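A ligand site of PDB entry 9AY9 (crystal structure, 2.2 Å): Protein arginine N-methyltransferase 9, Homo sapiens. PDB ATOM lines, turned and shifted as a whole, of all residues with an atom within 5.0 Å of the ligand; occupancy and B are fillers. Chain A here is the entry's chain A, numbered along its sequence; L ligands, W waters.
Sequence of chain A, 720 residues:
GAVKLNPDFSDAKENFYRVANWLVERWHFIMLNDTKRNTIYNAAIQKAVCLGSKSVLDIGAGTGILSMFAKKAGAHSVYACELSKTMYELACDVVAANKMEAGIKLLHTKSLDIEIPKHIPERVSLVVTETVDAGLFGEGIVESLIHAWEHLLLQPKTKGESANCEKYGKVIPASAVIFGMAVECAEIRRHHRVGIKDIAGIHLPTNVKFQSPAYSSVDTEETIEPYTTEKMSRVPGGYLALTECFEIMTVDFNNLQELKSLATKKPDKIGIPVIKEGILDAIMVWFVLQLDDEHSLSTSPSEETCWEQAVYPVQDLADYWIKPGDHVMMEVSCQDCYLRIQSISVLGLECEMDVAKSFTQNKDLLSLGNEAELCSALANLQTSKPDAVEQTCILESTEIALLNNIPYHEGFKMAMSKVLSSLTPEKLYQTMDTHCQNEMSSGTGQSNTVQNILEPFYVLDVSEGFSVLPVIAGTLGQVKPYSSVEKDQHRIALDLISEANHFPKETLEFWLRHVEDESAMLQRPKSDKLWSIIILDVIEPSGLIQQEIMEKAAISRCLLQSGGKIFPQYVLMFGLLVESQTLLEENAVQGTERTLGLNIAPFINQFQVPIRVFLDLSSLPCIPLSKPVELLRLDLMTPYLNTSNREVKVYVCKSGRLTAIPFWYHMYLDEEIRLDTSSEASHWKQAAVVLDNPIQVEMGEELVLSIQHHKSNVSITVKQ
Water W2 lies within hydrogen-bond range of the backbone carbonyl oxygen (O) of Glu 130 (2.7 Å) and a nitrogen (N5) of the ligand (3.4 Å).
The side-chain carboxylate (OE2) of Glu 82 lies within hydrogen-bond range of an oxygen (O1) of the ligand, 2.6 Å away. N3 of the ligand is in hydrogen-bond range of N of Ser 111, at 2.8 Å. OG of Ser 111 lies within hydrogen-bond range of N2 of the ligand, 2.8 Å away. A nitrogen (N5) of the ligand sits at hydrogen-bond distance from the backbone carbonyl oxygen (O) of Val 132 (2.8 Å). N of Glu 308 is in hydrogen-bond range of N6 of the ligand, at 3.0 Å. N of Leu 83 is in hydrogen-bond range of N4 of the ligand. A nitrogen (N2) of the ligand is in hydrogen-bond range of the side-chain hydroxyl (OG) of Ser 144, 3.4 Å away.
Trp 27 touches the ligand (NE1 to C15, 3.3 Å). Met 31 touches the ligand. Ile 59 touches the ligand. Gly 60 touches the ligand. O of Cys 81 touches C9 of the ligand, 3.8 Å away. N of Ser 84 touches O1 of the ligand, at 3.7 Å. Thr 109 touches the ligand. CG of Lys 110 touches N2 of the ligand, at 3.4 Å. Thr 131 touches the ligand (CG2 to C6, 3.6 Å). Asp 133 touches the ligand. Ala 134 touches the ligand. O of Glu 139 touches C7 of the ligand (3.1 Å). Cys 306 touches the ligand. Trp 307 touches the ligand (CE3 to C24, 3.6 Å). Hydrophobic or aromatic side chains that line the ligand: Trp 27, Met 31, Ile 59, Leu 83 and Trp 307. 20 residues have an atom within 4 Å of the ligand: Trp 27, Met 31, Ile 59, Gly 60, Cys 81, Glu 82, Leu 83, Ser 84, Thr 109, Lys 110, Ser 111, Thr 131, Val 132, Asp 133, Ala 134, Glu 139, Ser 144, Cys 306, Trp 307 and Glu 308. The nearest printed residue that does not touch the ligand is Glu 130 (4.2 Å).
The backbone NH (N) of Thr 109 sits at hydrogen-bond distance from the backbone carbonyl oxygen (O) of Glu 82, 3.2 Å away. The side-chain carboxylate (OE2) of Glu 82 lies within hydrogen-bond range of the backbone NH (N) of Ser 84, at 2.8 Å. The side-chain carboxylate (OE1) of Glu 82 is in hydrogen-bond range of the backbone NH (N) of Gly 62 (2.9 Å). The backbone NH (N) of Leu 83 sits at hydrogen-bond distance from the backbone carbonyl oxygen (O) of Thr 109 (3.3 Å). N of Gly 60 lies within hydrogen-bond range of O of Cys 81 (3.0 Å). OG of Ser 84 lies within hydrogen-bond range of N of Met 87 (3.2 Å). The backbone carbonyl oxygen (O) of Cys 81 sits at hydrogen-bond distance from the backbone NH (N) of Ala 61.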
ATOM      1  N   TRP A  27      -1.190   4.811  25.122  1.00  0.00           N
ATOM      2  CA  TRP A  27      -1.478   3.952  23.965  1.00  0.00           C
ATOM      3  C   TRP A  27      -0.860   4.480  22.660  1.00  0.00           C
ATOM      4  O   TRP A  27      -0.672   3.677  21.746  1.00  0.00           O
ATOM      5  CB  TRP A  27      -2.985   3.726  23.769  1.00  0.00           C
ATOM      6  CG  TRP A  27      -3.840   4.957  23.741  1.00  0.00           C
ATOM      7  CD1 TRP A  27      -3.998   5.842  22.709  1.00  0.00           C
ATOM      8  CD2 TRP A  27      -4.744   5.370  24.764  1.00  0.00           C
ATOM      9  NE1 TRP A  27      -4.916   6.800  23.049  1.00  0.00           N
ATOM     10  CE2 TRP A  27      -5.424   6.516  24.291  1.00  0.00           C
ATOM     11  CE3 TRP A  27      -5.034   4.908  26.062  1.00  0.00           C
ATOM     12  CZ2 TRP A  27      -6.390   7.180  25.054  1.00  0.00           C
ATOM     13  CZ3 TRP A  27      -5.977   5.579  26.829  1.00  0.00           C
ATOM     14  CH2 TRP A  27      -6.644   6.712  26.325  1.00  0.00           C
ATOM     15  N   HIS A  28      -0.537   5.782  22.556  1.00  0.00           N
ATOM     16  CA  HIS A  28       0.097   6.326  21.349  1.00  0.00           C
ATOM     17  C   HIS A  28       1.486   5.736  21.119  1.00  0.00           C
ATOM     18  O   HIS A  28       1.827   5.446  19.980  1.00  0.00           O
ATOM     19  CB  HIS A  28       0.188   7.866  21.388  1.00  0.00           C
ATOM     20  CG  HIS A  28      -1.142   8.564  21.282  1.00  0.00           C
ATOM     21  ND1 HIS A  28      -1.900   8.498  20.126  1.00  0.00           N
ATOM     22  CD2 HIS A  28      -1.770   9.355  22.183  1.00  0.00           C
ATOM     23  CE1 HIS A  28      -2.976   9.220  20.372  1.00  0.00           C
ATOM     24  NE2 HIS A  28      -2.950   9.766  21.586  1.00  0.00           N
ATOM     25  N   MET A  31       1.100   1.795  19.950  1.00  0.00           N
ATOM     26  CA  MET A  31       0.578   1.747  18.588  1.00  0.00           C
ATOM     27  C   MET A  31       1.632   2.144  17.556  1.00  0.00           C
ATOM     28  O   MET A  31       1.793   1.439  16.558  1.00  0.00           O
ATOM     29  CB  MET A  31      -0.662   2.642  18.447  1.00  0.00           C
ATOM     30  CG  MET A  31      -1.882   2.123  19.166  1.00  0.00           C
ATOM     31  SD  MET A  31      -3.416   2.976  18.683  1.00  0.00           S
ATOM     32  CE  MET A  31      -3.225   4.553  19.513  1.00  0.00           C
ATOM     33  N   ILE A  59      -9.670  11.396  10.238  1.00  0.00           N
ATOM     34  CA  ILE A  59     -10.466  11.701  11.422  1.00  0.00           C
ATOM     35  C   ILE A  59      -9.759  11.148  12.647  1.00  0.00           C
ATOM     36  O   ILE A  59      -9.654   9.935  12.801  1.00  0.00           O
ATOM     37  CB  ILE A  59     -11.943  11.220  11.321  1.00  0.00           C
ATOM     38  CG1 ILE A  59     -12.675  11.926  10.149  1.00  0.00           C
ATOM     39  CG2 ILE A  59     -12.676  11.466  12.664  1.00  0.00           C
ATOM     40  CD1 ILE A  59     -14.127  11.391   9.835  1.00  0.00           C
ATOM     41  N   GLY A  60      -9.324  12.069  13.511  1.00  0.00           N
ATOM     42  CA  GLY A  60      -8.603  11.765  14.743  1.00  0.00           C
ATOM     43  C   GLY A  60      -7.162  11.402  14.447  1.00  0.00           C
ATOM     44  O   GLY A  60      -6.695  10.325  14.810  1.00  0.00           O
ATOM     45  N   ALA A  61      -6.464  12.330  13.776  1.00  0.00           N
ATOM     46  CA  ALA A  61      -5.098  12.240  13.241  1.00  0.00           C
ATOM     47  C   ALA A  61      -3.987  11.851  14.257  1.00  0.00           C
ATOM     48  O   ALA A  61      -2.981  11.310  13.812  1.00  0.00           O
ATOM     49  CB  ALA A  61      -4.710  13.558  12.586  1.00  0.00           C
ATOM     50  N   GLY A  62      -4.135  12.155  15.548  1.00  0.00           N
ATOM     51  CA  GLY A  62      -3.105  11.858  16.543  1.00  0.00           C
ATOM     52  C   GLY A  62      -1.833  12.620  16.182  1.00  0.00           C
ATOM     53  O   GLY A  62      -1.878  13.850  16.054  1.00  0.00           O
ATOM     54  N   CYS A  81      -7.889  16.099  10.988  1.00  0.00           N
ATOM     55  CA  CYS A  81      -8.508  16.774  12.108  1.00  0.00           C
ATOM     56  C   CYS A  81      -8.192  16.055  13.402  1.00  0.00           C
ATOM     57  O   CYS A  81      -8.120  14.826  13.453  1.00  0.00           O
ATOM     58  CB  CYS A  81     -10.007  16.985  11.909  1.00  0.00           C
ATOM     59  SG  CYS A  81     -10.969  15.453  11.839  1.00  0.00           S
ATOM     60  N   GLU A  82      -7.952  16.858  14.440  1.00  0.00           N
ATOM     61  CA  GLU A  82      -7.614  16.355  15.753  1.00  0.00           C
ATOM     62  C   GLU A  82      -8.309  17.196  16.827  1.00  0.00           C
ATOM     63  O   GLU A  82      -8.120  18.408  16.914  1.00  0.00           O
ATOM     64  CB  GLU A  82      -6.078  16.308  15.928  1.00  0.00           C
ATOM     65  CG  GLU A  82      -5.601  15.847  17.288  1.00  0.00           C
ATOM     66  CD  GLU A  82      -6.271  14.605  17.828  1.00  0.00           C
ATOM     67  OE1 GLU A  82      -6.062  13.511  17.257  1.00  0.00           O
ATOM     68  OE2 GLU A  82      -7.007  14.722  18.827  1.00  0.00           O
ATOM     69  N   LEU A  83      -9.147  16.518  17.610  1.00  0.00           N
ATOM     70  CA  LEU A  83      -9.942  17.002  18.733  1.00  0.00           C
ATOM     71  C   LEU A  83      -9.030  17.652  19.826  1.00  0.00           C
ATOM     72  O   LEU A  83      -9.261  18.810  20.225  1.00  0.00           O
ATOM     73  CB  LEU A  83     -10.666  15.752  19.292  1.00  0.00           C
ATOM     74  CG  LEU A  83     -11.773  15.904  20.276  1.00  0.00           C
ATOM     75  CD1 LEU A  83     -12.809  14.843  20.022  1.00  0.00           C
ATOM     76  CD2 LEU A  83     -11.242  15.778  21.708  1.00  0.00           C
ATOM     77  N   SER A  84      -8.017  16.894  20.302  1.00  0.00           N
ATOM     78  CA  SER A  84      -7.051  17.263  21.330  1.00  0.00           C
ATOM     79  C   SER A  84      -6.109  18.375  20.893  1.00  0.00           C
ATOM     80  O   SER A  84      -5.483  18.256  19.836  1.00  0.00           O
ATOM     81  CB  SER A  84      -6.261  16.024  21.757  1.00  0.00           C
ATOM     82  OG  SER A  84      -5.083  16.322  22.496  1.00  0.00           O
ATOM     83  N   MET A  87      -2.382  16.892  20.951  1.00  0.00           N
ATOM     84  CA  MET A  87      -2.116  16.041  19.784  1.00  0.00           C
ATOM     85  C   MET A  87      -2.053  16.862  18.517  1.00  0.00           C
ATOM     86  O   MET A  87      -1.172  16.618  17.693  1.00  0.00           O
ATOM     87  CB  MET A  87      -3.135  14.892  19.654  1.00  0.00           C
ATOM     88  CG  MET A  87      -3.085  13.868  20.798  1.00  0.00           C
ATOM     89  SD  MET A  87      -1.427  13.234  21.229  1.00  0.00           S
ATOM     90  CE  MET A  87      -0.967  12.323  19.683  1.00  0.00           C
ATOM     91  N   THR A 109     -10.044  20.597  15.669  1.00  0.00           N
ATOM     92  CA  THR A 109     -11.503  20.447  15.774  1.00  0.00           C
ATOM     93  C   THR A 109     -11.906  18.976  15.840  1.00  0.00           C
ATOM     94  O   THR A 109     -11.131  18.095  15.443  1.00  0.00           O
ATOM     95  CB  THR A 109     -12.226  21.170  14.570  1.00  0.00           C
ATOM     96  OG1 THR A 109     -13.643  20.986  14.672  1.00  0.00           O
ATOM     97  CG2 THR A 109     -11.764  20.681  13.196  1.00  0.00           C
ATOM     98  N   LYS A 110     -13.130  18.723  16.280  1.00  0.00           N
ATOM     99  CA  LYS A 110     -13.729  17.409  16.188  1.00  0.00           C
ATOM    100  C   LYS A 110     -14.249  17.408  14.738  1.00  0.00           C
ATOM    101  O   LYS A 110     -14.616  18.460  14.219  1.00  0.00           O
ATOM    102  CB  LYS A 110     -14.889  17.255  17.206  1.00  0.00           C
ATOM    103  CG  LYS A 110     -15.484  15.850  17.198  1.00  0.00           C
ATOM    104  CD  LYS A 110     -16.120  15.428  18.517  1.00  0.00           C
ATOM    105  CE  LYS A 110     -16.422  13.947  18.453  1.00  0.00           C
ATOM    106  NZ  LYS A 110     -16.798  13.361  19.760  1.00  0.00           N
ATOM    107  N   SER A 111     -14.268  16.239  14.067  1.00  0.00           N
ATOM    108  CA  SER A 111     -14.717  16.116  12.667  1.00  0.00           C
ATOM    109  C   SER A 111     -16.188  16.550  12.486  1.00  0.00           C
ATOM    110  O   SER A 111     -16.569  16.968  11.387  1.00  0.00           O
ATOM    111  CB  SER A 111     -14.513  14.691  12.171  1.00  0.00           C
ATOM    112  OG  SER A 111     -15.291  13.767  12.918  1.00  0.00           O
ATOM    113  N   LEU A 112     -16.992  16.455  13.573  1.00  0.00           N
ATOM    114  CA  LEU A 112     -18.413  16.817  13.596  1.00  0.00           C
ATOM    115  C   LEU A 112     -18.631  18.304  13.374  1.00  0.00           C
ATOM    116  O   LEU A 112     -19.711  18.703  12.934  1.00  0.00           O
ATOM    117  CB  LEU A 112     -19.092  16.392  14.920  1.00  0.00           C
ATOM    118  CG  LEU A 112     -18.964  14.939  15.396  1.00  0.00           C
ATOM    119  CD1 LEU A 112     -19.598  14.751  16.747  1.00  0.00           C
ATOM    120  CD2 LEU A 112     -19.581  13.970  14.422  1.00  0.00           C
ATOM    121  N   GLU A 130      -8.962   5.876  12.879  1.00  0.00           N
ATOM    122  CA  GLU A 130      -8.506   4.884  13.834  1.00  0.00           C
ATOM    123  C   GLU A 130      -9.166   5.121  15.191  1.00  0.00           C
ATOM    124  O   GLU A 130      -8.667   4.668  16.224  1.00  0.00           O
ATOM    125  CB  GLU A 130      -7.007   5.037  14.002  1.00  0.00           C
ATOM    126  CG  GLU A 130      -6.225   4.294  12.955  1.00  0.00           C
ATOM    127  CD  GLU A 130      -4.879   4.005  13.556  1.00  0.00           C
ATOM    128  OE1 GLU A 130      -3.963   4.851  13.398  1.00  0.00           O
ATOM    129  OE2 GLU A 130      -4.766   2.962  14.240  1.00  0.00           O
ATOM    130  N   THR A 131     -10.290   5.860  15.172  1.00  0.00           N
ATOM    131  CA  THR A 131     -11.079   6.249  16.344  1.00  0.00           C
ATOM    132  C   THR A 131     -11.884   5.037  16.812  1.00  0.00           C
ATOM    133  O   THR A 131     -13.122   5.050  16.768  1.00  0.00           O
ATOM    134  CB  THR A 131     -11.955   7.485  16.016  1.00  0.00           C
ATOM    135  OG1 THR A 131     -12.771   7.182  14.882  1.00  0.00           O
ATOM    136  CG2 THR A 131     -11.142   8.763  15.751  1.00  0.00           C
ATOM    137  N   VAL A 132     -11.181   3.975  17.232  1.00  0.00           N
ATOM    138  CA  VAL A 132     -11.781   2.737  17.737  1.00  0.00           C
ATOM    139  C   VAL A 132     -11.127   2.350  19.071  1.00  0.00           C
ATOM    140  O   VAL A 132      -9.945   2.612  19.302  1.00  0.00           O
ATOM    141  CB  VAL A 132     -11.766   1.541  16.735  1.00  0.00           C
ATOM    142  CG1 VAL A 132     -12.512   1.876  15.443  1.00  0.00           C
ATOM    143  CG2 VAL A 132     -10.351   1.043  16.444  1.00  0.00           C
ATOM    144  N   ASP A 133     -11.916   1.712  19.947  1.00  0.00           N
ATOM    145  CA  ASP A 133     -11.417   1.190  21.193  1.00  0.00           C
ATOM    146  C   ASP A 133     -11.494  -0.348  21.149  1.00  0.00           C
ATOM    147  O   ASP A 133     -11.756  -0.900  20.078  1.00  0.00           O
ATOM    148  CB  ASP A 133     -12.153   1.798  22.405  1.00  0.00           C
ATOM    149  CG  ASP A 133     -13.576   1.324  22.639  1.00  0.00           C
ATOM    150  OD1 ASP A 133     -14.232   0.869  21.668  1.00  0.00           O
ATOM    151  OD2 ASP A 133     -14.045   1.433  23.777  1.00  0.00           O
ATOM    152  N   ALA A 134     -11.260  -1.017  22.311  1.00  0.00           N
ATOM    153  CA  ALA A 134     -11.333  -2.486  22.461  1.00  0.00           C
ATOM    154  C   ALA A 134     -12.745  -3.030  22.130  1.00  0.00           C
ATOM    155  O   ALA A 134     -12.852  -4.144  21.617  1.00  0.00           O
ATOM    156  CB  ALA A 134     -10.915  -2.869  23.876  1.00  0.00           C
ATOM    157  N   GLU A 139     -15.292   4.983  20.849  1.00  0.00           N
ATOM    158  CA  GLU A 139     -14.771   6.307  20.543  1.00  0.00           C
ATOM    159  C   GLU A 139     -15.728   7.080  19.619  1.00  0.00           C
ATOM    160  O   GLU A 139     -15.333   8.096  19.065  1.00  0.00           O
ATOM    161  CB  GLU A 139     -13.342   6.241  19.936  1.00  0.00           C
ATOM    162  CG  GLU A 139     -12.290   5.609  20.841  1.00  0.00           C
ATOM    163  CD  GLU A 139     -12.010   6.262  22.176  1.00  0.00           C
ATOM    164  OE1 GLU A 139     -11.667   5.520  23.122  1.00  0.00           O
ATOM    165  OE2 GLU A 139     -12.105   7.503  22.281  1.00  0.00           O
ATOM    166  N   SER A 144     -19.419   9.777  14.113  1.00  0.00           N
ATOM    167  CA  SER A 144     -18.462  10.470  13.266  1.00  0.00           C
ATOM    168  C   SER A 144     -18.591  10.077  11.769  1.00  0.00           C
ATOM    169  O   SER A 144     -18.525  10.951  10.903  1.00  0.00           O
ATOM    170  CB  SER A 144     -17.041  10.219  13.749  1.00  0.00           C
ATOM    171  OG  SER A 144     -16.865  10.710  15.068  1.00  0.00           O
ATOM    172  N   PHE A 287     -12.465  -7.921  17.734  1.00  0.00           N
ATOM    173  CA  PHE A 287     -13.016  -7.737  16.403  1.00  0.00           C
ATOM    174  C   PHE A 287     -11.957  -7.918  15.308  1.00  0.00           C
ATOM    175  O   PHE A 287     -10.754  -7.790  15.548  1.00  0.00           O
ATOM    176  CB  PHE A 287     -13.700  -6.353  16.274  1.00  0.00           C
ATOM    177  CG  PHE A 287     -12.836  -5.147  16.590  1.00  0.00           C
ATOM    178  CD1 PHE A 287     -12.741  -4.654  17.895  1.00  0.00           C
ATOM    179  CD2 PHE A 287     -12.132  -4.483  15.588  1.00  0.00           C
ATOM    180  CE1 PHE A 287     -11.940  -3.553  18.184  1.00  0.00           C
ATOM    181  CE2 PHE A 287     -11.328  -3.384  15.885  1.00  0.00           C
ATOM    182  CZ  PHE A 287     -11.256  -2.912  17.183  1.00  0.00           C
ATOM    183  N   THR A 299      -8.030  -7.868  16.555  1.00  0.00           N
ATOM    184  CA  THR A 299      -7.751  -7.500  17.955  1.00  0.00           C
ATOM    185  C   THR A 299      -7.867  -8.734  18.840  1.00  0.00           C
ATOM    186  O   THR A 299      -7.962  -8.621  20.057  1.00  0.00           O
ATOM    187  CB  THR A 299      -8.610  -6.310  18.470  1.00  0.00           C
ATOM    188  OG1 THR A 299      -9.987  -6.698  18.544  1.00  0.00           O
ATOM    189  CG2 THR A 299      -8.451  -5.057  17.630  1.00  0.00           C
ATOM    190  N   CYS A 306      -0.502  -5.472  19.957  1.00  0.00           N
ATOM    191  CA  CYS A 306      -0.695  -4.414  20.955  1.00  0.00           C
ATOM    192  C   CYS A 306      -2.149  -4.318  21.458  1.00  0.00           C
ATOM    193  O   CYS A 306      -2.391  -3.648  22.467  1.00  0.00           O
ATOM    194  CB  CYS A 306      -0.241  -3.084  20.367  1.00  0.00           C
ATOM    195  SG  CYS A 306      -1.377  -2.383  19.137  1.00  0.00           S
ATOM    196  N   TRP A 307      -3.099  -4.922  20.735  1.00  0.00           N
ATOM    197  CA  TRP A 307      -4.520  -4.797  20.991  1.00  0.00           C
ATOM    198  C   TRP A 307      -5.001  -5.427  22.282  1.00  0.00           C
ATOM    199  O   TRP A 307      -4.665  -6.565  22.612  1.00  0.00           O
ATOM    200  CB  TRP A 307      -5.328  -5.394  19.828  1.00  0.00           C
ATOM    201  CG  TRP A 307      -4.892  -4.925  18.476  1.00  0.00           C
ATOM    202  CD1 TRP A 307      -4.336  -5.686  17.489  1.00  0.00           C
ATOM    203  CD2 TRP A 307      -4.895  -3.575  17.991  1.00  0.00           C
ATOM    204  NE1 TRP A 307      -3.991  -4.883  16.420  1.00  0.00           N
ATOM    205  CE2 TRP A 307      -4.344  -3.589  16.693  1.00  0.00           C
ATOM    206  CE3 TRP A 307      -5.333  -2.345  18.521  1.00  0.00           C
ATOM    207  CZ2 TRP A 307      -4.228  -2.428  15.910  1.00  0.00           C
ATOM    208  CZ3 TRP A 307      -5.190  -1.192  17.770  1.00  0.00           C
ATOM    209  CH2 TRP A 307      -4.670  -1.245  16.473  1.00  0.00           C
ATOM    210  N   GLU A 308      -5.872  -4.664  22.969  1.00  0.00           N
ATOM    211  CA  GLU A 308      -6.584  -5.079  24.154  1.00  0.00           C
ATOM    212  C   GLU A 308      -7.998  -5.495  23.737  1.00  0.00           C
ATOM    213  O   GLU A 308      -8.456  -5.156  22.646  1.00  0.00           O
ATOM    214  CB  GLU A 308      -6.626  -3.963  25.199  1.00  0.00           C
ATOM    215  CG  GLU A 308      -5.319  -3.823  25.967  1.00  0.00           C
ATOM    216  CD  GLU A 308      -5.227  -2.626  26.905  1.00  0.00           C
ATOM    217  OE1 GLU A 308      -6.240  -1.909  27.049  1.00  0.00           O
ATOM    218  OE2 GLU A 308      -4.146  -2.422  27.501  1.00  0.00           O
HETATM  219  C1  LIG L   1      -7.977  -0.360  20.081  1.00  0.00           C
HETATM  220  C2  LIG L   1     -11.125  12.935  17.015  1.00  0.00           C
HETATM  221  C3  LIG L   1      -6.878   0.183  20.731  1.00  0.00           C
HETATM  222  C4  LIG L   1     -12.467  12.572  16.806  1.00  0.00           C
HETATM  223  C5  LIG L   1      -8.919  11.966  19.851  1.00  0.00           C
HETATM  224  C6  LIG L   1     -11.576  11.216  18.356  1.00  0.00           C
HETATM  225  C7  LIG L   1     -14.013  10.685  17.855  1.00  0.00           C
HETATM  226  C8  LIG L   1     -12.734  11.450  17.690  1.00  0.00           C
HETATM  227  C9  LIG L   1     -11.256  14.586  15.533  1.00  0.00           C
HETATM  228  C10 LIG L   1     -13.174  13.330  15.838  1.00  0.00           C
HETATM  229  C11 LIG L   1      -6.399   1.565  20.346  1.00  0.00           C
HETATM  230  C12 LIG L   1      -6.818   3.932  20.721  1.00  0.00           C
HETATM  231  C13 LIG L   1      -8.262   9.925  18.846  1.00  0.00           C
HETATM  232  O1  LIG L   1      -8.469  13.213  20.358  1.00  0.00           O
HETATM  233  C14 LIG L   1      -7.845   4.997  20.480  1.00  0.00           C
HETATM  234  C15 LIG L   1      -7.567   6.278  21.227  1.00  0.00           C
HETATM  235  C16 LIG L   1      -5.362   1.032  23.440  1.00  0.00           C
HETATM  236  C17 LIG L   1      -4.998  -0.214  22.601  1.00  0.00           C
HETATM  237  C18 LIG L   1      -8.684   7.279  21.069  1.00  0.00           C
HETATM  238  C19 LIG L   1      -3.774   0.101  21.725  1.00  0.00           C
HETATM  239  C20 LIG L   1      -7.828  10.881  19.941  1.00  0.00           C
HETATM  240  O2  LIG L   1      -6.522  11.371  19.635  1.00  0.00           O
HETATM  241  C21 LIG L   1      -9.174  12.016  18.337  1.00  0.00           C
HETATM  242  N1  LIG L   1     -10.592  12.086  17.946  1.00  0.00           N
HETATM  243  N2  LIG L   1     -14.454  13.107  15.512  1.00  0.00           N
HETATM  244  N3  LIG L   1     -12.532  14.347  15.212  1.00  0.00           N
HETATM  245  N4  LIG L   1     -10.476  13.947  16.407  1.00  0.00           N
HETATM  246  O3  LIG L   1      -8.631  10.827  17.778  1.00  0.00           O
HETATM  247  C22 LIG L   1      -9.542   9.181  19.193  1.00  0.00           C
HETATM  248  S1  LIG L   1      -9.208   7.439  19.345  1.00  0.00           S
HETATM  249  N5  LIG L   1      -7.407   2.606  20.522  1.00  0.00           N
HETATM  250  C23 LIG L   1      -8.379  -1.667  20.346  1.00  0.00           C
HETATM  251  C24 LIG L   1      -7.656  -2.401  21.282  1.00  0.00           C
HETATM  252  N6  LIG L   1      -6.591  -1.933  21.957  1.00  0.00           N
HETATM  253  C25 LIG L   1      -6.184  -0.680  21.730  1.00  0.00           C
HETATM  254  C26 LIG L   1      -4.586  -1.298  23.591  1.00  0.00           C
HETATM  255  O   HOH W   1     -15.010   9.973  21.034  1.00  0.00           O
HETATM  256  O   HOH W   2      -7.019   2.722  17.111  1.00  0.00           O
HETATM  257  O   HOH W   3      -8.628   2.390  23.006  1.00  0.00           O
